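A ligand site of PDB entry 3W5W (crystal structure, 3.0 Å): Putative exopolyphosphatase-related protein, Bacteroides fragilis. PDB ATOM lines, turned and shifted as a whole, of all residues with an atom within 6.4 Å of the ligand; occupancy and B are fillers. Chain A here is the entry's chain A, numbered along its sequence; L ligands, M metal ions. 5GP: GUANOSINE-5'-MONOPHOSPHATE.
O3P of the ligand is in hydrogen-bond range of OG of Ser 289, at 2.9 Å. A nitrogen (N7) of the ligand lies within hydrogen-bond range of the backbone NH of Gly 317 (3.4 Å). The guanidinium group of Arg 291 is in salt-bridge range of an oxygen (O3P) of the ligand (2.5 Å). O2' of the ligand sits at hydrogen-bond distance from NH1 of Arg 105, 3.1 Å away. An oxygen (O2P) of the ligand is in salt-bridge range of the side-chain amino group (NZ) of Lys 287.
ND1 of His 29 lies within hydrogen-bond range of NH2 of Arg 105 (3.4 Å). The backbone NH (N) of Ile 288 sits at hydrogen-bond distance from the backbone carbonyl oxygen (O) of Gly 317 (2.9 Å). The backbone NH (N) of Leu 290 lies within hydrogen-bond range of the backbone carbonyl oxygen (O) of Ser 315 (2.5 Å). The backbone NH (N) of Gly 316 is in hydrogen-bond range of the backbone carbonyl oxygen (O) of Gly 309 (3.4 Å). The side-chain amino group of Lys 287 lies within hydrogen-bond range of the side-chain hydroxyl of Ser 289 (3.0 Å).
The backbone carbonyl oxygen (O) of Gly 309 lies close to a nitrogen (N3) of the ligand (3.5 Å). Residues that only touch the ligand: Ser 315 (3.1 Å), Gly 316 (3.2 Å), Gly 308 (3.5 Å), Gly 310 (3.7 Å) and Ala 314 (3.9 Å).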
ATOM      1  N   HIS A  29       3.377  16.401 -36.144  1.00  0.00           N
ATOM      2  CA  HIS A  29       3.305  15.276 -35.206  1.00  0.00           C
ATOM      3  C   HIS A  29       2.102  14.333 -35.256  1.00  0.00           C
ATOM      4  O   HIS A  29       1.024  14.704 -35.709  1.00  0.00           O
ATOM      5  CB  HIS A  29       3.459  15.795 -33.778  1.00  0.00           C
ATOM      6  CG  HIS A  29       2.320  16.656 -33.329  1.00  0.00           C
ATOM      7  ND1 HIS A  29       1.108  16.134 -32.926  1.00  0.00           N
ATOM      8  CD2 HIS A  29       2.204  17.996 -33.227  1.00  0.00           C
ATOM      9  CE1 HIS A  29       0.297  17.117 -32.583  1.00  0.00           C
ATOM     10  NE2 HIS A  29       0.930  18.267 -32.765  1.00  0.00           N
ATOM     11  N   LYS A 104      10.699  11.148 -32.465  1.00  0.00           N
ATOM     12  CA  LYS A 104       9.767  10.187 -31.918  1.00  0.00           C
ATOM     13  C   LYS A 104       8.337  10.690 -32.039  1.00  0.00           C
ATOM     14  O   LYS A 104       7.400   9.908 -32.039  1.00  0.00           O
ATOM     15  CB  LYS A 104      10.092   9.898 -30.464  1.00  0.00           C
ATOM     16  CG  LYS A 104      10.110  11.129 -29.573  1.00  0.00           C
ATOM     17  CD  LYS A 104      10.280  10.763 -28.098  1.00  0.00           C
ATOM     18  CE  LYS A 104      10.342  11.993 -27.201  1.00  0.00           C
ATOM     19  NZ  LYS A 104      10.549  11.612 -25.768  1.00  0.00           N
ATOM     20  N   ARG A 105       8.189  12.002 -32.158  1.00  0.00           N
ATOM     21  CA  ARG A 105       6.883  12.637 -32.258  1.00  0.00           C
ATOM     22  C   ARG A 105       6.122  12.333 -33.536  1.00  0.00           C
ATOM     23  O   ARG A 105       4.888  12.332 -33.543  1.00  0.00           O
ATOM     24  CB  ARG A 105       7.036  14.150 -32.100  1.00  0.00           C
ATOM     25  CG  ARG A 105       7.392  14.576 -30.687  1.00  0.00           C
ATOM     26  CD  ARG A 105       6.284  14.196 -29.757  1.00  0.00           C
ATOM     27  NE  ARG A 105       5.072  14.909 -30.107  1.00  0.00           N
ATOM     28  CZ  ARG A 105       3.854  14.475 -29.801  1.00  0.00           C
ATOM     29  NH1 ARG A 105       3.710  13.336 -29.151  1.00  0.00           N
ATOM     30  NH2 ARG A 105       2.787  15.185 -30.159  1.00  0.00           N
ATOM     31  N   HIS A 126       7.790  23.850 -28.422  1.00  0.00           N
ATOM     32  CA  HIS A 126       7.764  22.945 -27.285  1.00  0.00           C
ATOM     33  C   HIS A 126       9.147  22.986 -26.620  1.00  0.00           C
ATOM     34  O   HIS A 126      10.117  23.378 -27.253  1.00  0.00           O
ATOM     35  CB  HIS A 126       7.415  21.538 -27.783  1.00  0.00           C
ATOM     36  CG  HIS A 126       5.997  21.430 -28.253  1.00  0.00           C
ATOM     37  ND1 HIS A 126       4.950  21.135 -27.410  1.00  0.00           N
ATOM     38  CD2 HIS A 126       5.445  21.637 -29.474  1.00  0.00           C
ATOM     39  CE1 HIS A 126       3.811  21.178 -28.084  1.00  0.00           C
ATOM     40  NE2 HIS A 126       4.091  21.476 -29.342  1.00  0.00           N
ATOM     41  N   GLU A 259     -13.226  14.345 -26.296  1.00  0.00           N
ATOM     42  CA  GLU A 259     -12.203  15.369 -26.487  1.00  0.00           C
ATOM     43  C   GLU A 259     -12.478  16.551 -25.555  1.00  0.00           C
ATOM     44  O   GLU A 259     -13.634  16.891 -25.295  1.00  0.00           O
ATOM     45  CB  GLU A 259     -12.215  15.866 -27.932  1.00  0.00           C
ATOM     46  CG  GLU A 259     -11.154  16.914 -28.252  1.00  0.00           C
ATOM     47  CD  GLU A 259      -9.761  16.316 -28.400  1.00  0.00           C
ATOM     48  OE1 GLU A 259      -9.319  15.583 -27.485  1.00  0.00           O
ATOM     49  OE2 GLU A 259      -9.107  16.587 -29.435  1.00  0.00           O
ATOM     50  N   VAL A 262     -11.454  16.229 -20.278  1.00  0.00           N
ATOM     51  CA  VAL A 262     -10.540  16.315 -19.141  1.00  0.00           C
ATOM     52  C   VAL A 262     -10.358  17.755 -18.647  1.00  0.00           C
ATOM     53  O   VAL A 262      -9.912  17.987 -17.522  1.00  0.00           O
ATOM     54  CB  VAL A 262      -9.164  15.727 -19.515  1.00  0.00           C
ATOM     55  CG1 VAL A 262      -8.570  16.501 -20.669  1.00  0.00           C
ATOM     56  CG2 VAL A 262      -8.239  15.758 -18.313  1.00  0.00           C
ATOM     57  N   LYS A 287      -7.132   4.296 -20.643  1.00  0.00           N
ATOM     58  CA  LYS A 287      -6.504   5.452 -21.284  1.00  0.00           C
ATOM     59  C   LYS A 287      -6.538   6.669 -20.349  1.00  0.00           C
ATOM     60  O   LYS A 287      -7.613   7.215 -20.073  1.00  0.00           O
ATOM     61  CB  LYS A 287      -7.213   5.789 -22.603  1.00  0.00           C
ATOM     62  CG  LYS A 287      -6.768   7.100 -23.262  1.00  0.00           C
ATOM     63  CD  LYS A 287      -5.334   7.043 -23.771  1.00  0.00           C
ATOM     64  CE  LYS A 287      -4.398   7.915 -22.942  1.00  0.00           C
ATOM     65  NZ  LYS A 287      -4.719   9.378 -23.016  1.00  0.00           N
ATOM     66  N   ILE A 288      -5.367   7.077 -19.879  1.00  0.00           N
ATOM     67  CA  ILE A 288      -5.232   8.219 -18.974  1.00  0.00           C
ATOM     68  C   ILE A 288      -4.886   9.542 -19.655  1.00  0.00           C
ATOM     69  O   ILE A 288      -3.980   9.621 -20.491  1.00  0.00           O
ATOM     70  CB  ILE A 288      -4.155   7.940 -17.867  1.00  0.00           C
ATOM     71  CG1 ILE A 288      -4.664   6.922 -16.856  1.00  0.00           C
ATOM     72  CG2 ILE A 288      -3.789   9.231 -17.149  1.00  0.00           C
ATOM     73  CD1 ILE A 288      -4.780   5.517 -17.394  1.00  0.00           C
ATOM     74  N   SER A 289      -5.617  10.588 -19.291  1.00  0.00           N
ATOM     75  CA  SER A 289      -5.392  11.931 -19.825  1.00  0.00           C
ATOM     76  C   SER A 289      -5.316  12.869 -18.629  1.00  0.00           C
ATOM     77  O   SER A 289      -6.203  12.886 -17.780  1.00  0.00           O
ATOM     78  CB  SER A 289      -6.516  12.357 -20.756  1.00  0.00           C
ATOM     79  OG  SER A 289      -6.424  11.677 -21.991  1.00  0.00           O
ATOM     80  N   LEU A 290      -4.223  13.628 -18.558  1.00  0.00           N
ATOM     81  CA  LEU A 290      -4.013  14.556 -17.473  1.00  0.00           C
ATOM     82  C   LEU A 290      -4.013  16.000 -17.930  1.00  0.00           C
ATOM     83  O   LEU A 290      -3.446  16.338 -18.973  1.00  0.00           O
ATOM     84  CB  LEU A 290      -2.695  14.240 -16.760  1.00  0.00           C
ATOM     85  CG  LEU A 290      -2.576  12.883 -16.072  1.00  0.00           C
ATOM     86  CD1 LEU A 290      -1.318  12.885 -15.211  1.00  0.00           C
ATOM     87  CD2 LEU A 290      -3.803  12.600 -15.200  1.00  0.00           C
ATOM     88  N   ARG A 291      -4.653  16.856 -17.145  1.00  0.00           N
ATOM     89  CA  ARG A 291      -4.728  18.273 -17.460  1.00  0.00           C
ATOM     90  C   ARG A 291      -4.602  19.042 -16.151  1.00  0.00           C
ATOM     91  O   ARG A 291      -5.009  18.550 -15.093  1.00  0.00           O
ATOM     92  CB  ARG A 291      -6.073  18.586 -18.119  1.00  0.00           C
ATOM     93  CG  ARG A 291      -6.018  19.717 -19.150  1.00  0.00           C
ATOM     94  CD  ARG A 291      -6.239  19.199 -20.555  1.00  0.00           C
ATOM     95  NE  ARG A 291      -5.327  18.115 -20.898  1.00  0.00           N
ATOM     96  CZ  ARG A 291      -5.406  17.370 -22.001  1.00  0.00           C
ATOM     97  NH1 ARG A 291      -4.527  16.419 -22.213  1.00  0.00           N
ATOM     98  NH2 ARG A 291      -6.378  17.592 -22.879  1.00  0.00           N
ATOM     99  N   PHE A 306       1.711   6.198 -15.071  1.00  0.00           N
ATOM    100  CA  PHE A 306       1.011   5.651 -16.232  1.00  0.00           C
ATOM    101  C   PHE A 306       1.853   5.536 -17.509  1.00  0.00           C
ATOM    102  O   PHE A 306       1.356   5.765 -18.602  1.00  0.00           O
ATOM    103  CB  PHE A 306      -0.249   6.496 -16.533  1.00  0.00           C
ATOM    104  CG  PHE A 306      -1.149   6.720 -15.330  1.00  0.00           C
ATOM    105  CD1 PHE A 306      -1.046   7.885 -14.573  1.00  0.00           C
ATOM    106  CD2 PHE A 306      -2.080   5.763 -14.948  1.00  0.00           C
ATOM    107  CE1 PHE A 306      -1.871   8.089 -13.456  1.00  0.00           C
ATOM    108  CE2 PHE A 306      -2.906   5.957 -13.829  1.00  0.00           C
ATOM    109  CZ  PHE A 306      -2.796   7.128 -13.087  1.00  0.00           C
ATOM    110  N   ASN A 307       3.110   5.149 -17.356  1.00  0.00           N
ATOM    111  CA  ASN A 307       4.045   4.978 -18.477  1.00  0.00           C
ATOM    112  C   ASN A 307       3.876   5.982 -19.613  1.00  0.00           C
ATOM    113  O   ASN A 307       3.774   5.597 -20.778  1.00  0.00           O
ATOM    114  CB  ASN A 307       3.919   3.567 -19.075  1.00  0.00           C
ATOM    115  CG  ASN A 307       3.982   2.482 -18.033  1.00  0.00           C
ATOM    116  OD1 ASN A 307       2.964   2.072 -17.477  1.00  0.00           O
ATOM    117  ND2 ASN A 307       5.196   1.996 -17.763  1.00  0.00           N
ATOM    118  N   GLY A 308       3.884   7.272 -19.291  1.00  0.00           N
ATOM    119  CA  GLY A 308       3.728   8.258 -20.340  1.00  0.00           C
ATOM    120  C   GLY A 308       4.657   9.445 -20.310  1.00  0.00           C
ATOM    121  O   GLY A 308       5.854   9.331 -20.021  1.00  0.00           O
ATOM    122  N   GLY A 309       4.086  10.603 -20.610  1.00  0.00           N
ATOM    123  CA  GLY A 309       4.845  11.839 -20.641  1.00  0.00           C
ATOM    124  C   GLY A 309       3.933  12.907 -21.201  1.00  0.00           C
ATOM    125  O   GLY A 309       2.707  12.749 -21.170  1.00  0.00           O
ATOM    126  N   GLY A 310       4.515  13.971 -21.736  1.00  0.00           N
ATOM    127  CA  GLY A 310       3.721  15.041 -22.295  1.00  0.00           C
ATOM    128  C   GLY A 310       4.233  16.389 -21.851  1.00  0.00           C
ATOM    129  O   GLY A 310       5.438  16.570 -21.695  1.00  0.00           O
ATOM    130  N   HIS A 311       3.336  17.344 -21.633  1.00  0.00           N
ATOM    131  CA  HIS A 311       3.724  18.685 -21.209  1.00  0.00           C
ATOM    132  C   HIS A 311       3.281  19.017 -19.792  1.00  0.00           C
ATOM    133  O   HIS A 311       2.526  18.282 -19.170  1.00  0.00           O
ATOM    134  CB  HIS A 311       3.158  19.709 -22.198  1.00  0.00           C
ATOM    135  CG  HIS A 311       3.427  19.366 -23.626  1.00  0.00           C
ATOM    136  ND1 HIS A 311       4.686  19.111 -24.109  1.00  0.00           N
ATOM    137  CD2 HIS A 311       2.578  19.176 -24.672  1.00  0.00           C
ATOM    138  CE1 HIS A 311       4.612  18.776 -25.384  1.00  0.00           C
ATOM    139  NE2 HIS A 311       3.346  18.812 -25.749  1.00  0.00           N
ATOM    140  N   ALA A 314      -0.632  19.427 -19.995  1.00  0.00           N
ATOM    141  CA  ALA A 314      -1.411  18.388 -20.674  1.00  0.00           C
ATOM    142  C   ALA A 314      -0.553  17.191 -21.057  1.00  0.00           C
ATOM    143  O   ALA A 314       0.541  17.337 -21.605  1.00  0.00           O
ATOM    144  CB  ALA A 314      -2.084  18.976 -21.906  1.00  0.00           C
ATOM    145  N   SER A 315      -1.056  15.996 -20.778  1.00  0.00           N
ATOM    146  CA  SER A 315      -0.320  14.775 -21.099  1.00  0.00           C
ATOM    147  C   SER A 315      -1.130  13.527 -20.719  1.00  0.00           C
ATOM    148  O   SER A 315      -2.118  13.621 -19.997  1.00  0.00           O
ATOM    149  CB  SER A 315       1.001  14.765 -20.334  1.00  0.00           C
ATOM    150  OG  SER A 315       0.787  14.935 -18.947  1.00  0.00           O
ATOM    151  N   GLY A 316      -0.702  12.365 -21.208  1.00  0.00           N
ATOM    152  CA  GLY A 316      -1.427  11.141 -20.908  1.00  0.00           C
ATOM    153  C   GLY A 316      -0.577   9.883 -20.813  1.00  0.00           C
ATOM    154  O   GLY A 316       0.570   9.914 -20.390  1.00  0.00           O
ATOM    155  N   GLY A 317      -1.170   8.767 -21.233  1.00  0.00           N
ATOM    156  CA  GLY A 317      -0.489   7.486 -21.191  1.00  0.00           C
ATOM    157  C   GLY A 317      -1.468   6.401 -20.760  1.00  0.00           C
ATOM    158  O   GLY A 317      -2.530   6.719 -20.222  1.00  0.00           O
ATOM    159  N   GLU A 318      -1.123   5.143 -20.987  1.00  0.00           N
ATOM    160  CA  GLU A 318      -2.025   4.057 -20.616  1.00  0.00           C
ATOM    161  C   GLU A 318      -1.605   3.237 -19.387  1.00  0.00           C
ATOM    162  O   GLU A 318      -0.424   3.109 -19.077  1.00  0.00           O
ATOM    163  CB  GLU A 318      -2.248   3.102 -21.799  1.00  0.00           C
ATOM    164  CG  GLU A 318      -3.183   1.920 -21.479  1.00  0.00           C
ATOM    165  CD  GLU A 318      -3.808   1.273 -22.717  1.00  0.00           C
ATOM    166  OE1 GLU A 318      -3.059   0.718 -23.552  1.00  0.00           O
ATOM    167  OE2 GLU A 318      -5.050   1.313 -22.840  1.00  0.00           O
HETATM  168  P   5GP L   1      -4.196  13.843 -24.184  1.00  0.00           P
HETATM  169  O1P 5GP L   1      -4.947  14.483 -25.292  1.00  0.00           O
HETATM  170  O2P 5GP L   1      -4.022  12.264 -24.485  1.00  0.00           O
HETATM  171  O3P 5GP L   1      -5.005  14.025 -22.805  1.00  0.00           O
HETATM  172  O5' 5GP L   1      -2.736  14.545 -24.033  1.00  0.00           O
HETATM  173  C5' 5GP L   1      -2.029  14.369 -25.268  1.00  0.00           C
HETATM  174  C4' 5GP L   1      -0.632  14.997 -25.174  1.00  0.00           C
HETATM  175  O4' 5GP L   1       0.138  14.390 -24.092  1.00  0.00           O
HETATM  176  C3' 5GP L   1       0.141  14.803 -26.493  1.00  0.00           C
HETATM  177  O3' 5GP L   1       0.547  16.063 -27.049  1.00  0.00           O
HETATM  178  C2' 5GP L   1       1.349  13.898 -26.158  1.00  0.00           C
HETATM  179  O2' 5GP L   1       2.582  14.533 -26.488  1.00  0.00           O
HETATM  180  C1' 5GP L   1       1.244  13.596 -24.644  1.00  0.00           C
HETATM  181  N9  5GP L   1       1.041  12.133 -24.382  1.00  0.00           N
HETATM  182  C8  5GP L   1      -0.166  11.478 -24.264  1.00  0.00           C
HETATM  183  N7  5GP L   1       0.025  10.206 -24.028  1.00  0.00           N
HETATM  184  C5  5GP L   1       1.357   9.960 -23.982  1.00  0.00           C
HETATM  185  C6  5GP L   1       2.143   8.783 -23.765  1.00  0.00           C
HETATM  186  O6  5GP L   1       1.614   7.704 -23.561  1.00  0.00           O
HETATM  187  N1  5GP L   1       3.515   8.892 -23.781  1.00  0.00           N
HETATM  188  C2  5GP L   1       4.125  10.115 -24.006  1.00  0.00           C
HETATM  189  N2  5GP L   1       5.495  10.195 -24.014  1.00  0.00           N
HETATM  190  N3  5GP L   1       3.397  11.220 -24.204  1.00  0.00           N
HETATM  191  C4  5GP L   1       2.031  11.188 -24.210  1.00  0.00           C
HETATM  192 MN    MN M   1       0.396  20.476 -31.447  1.00  0.00          MN
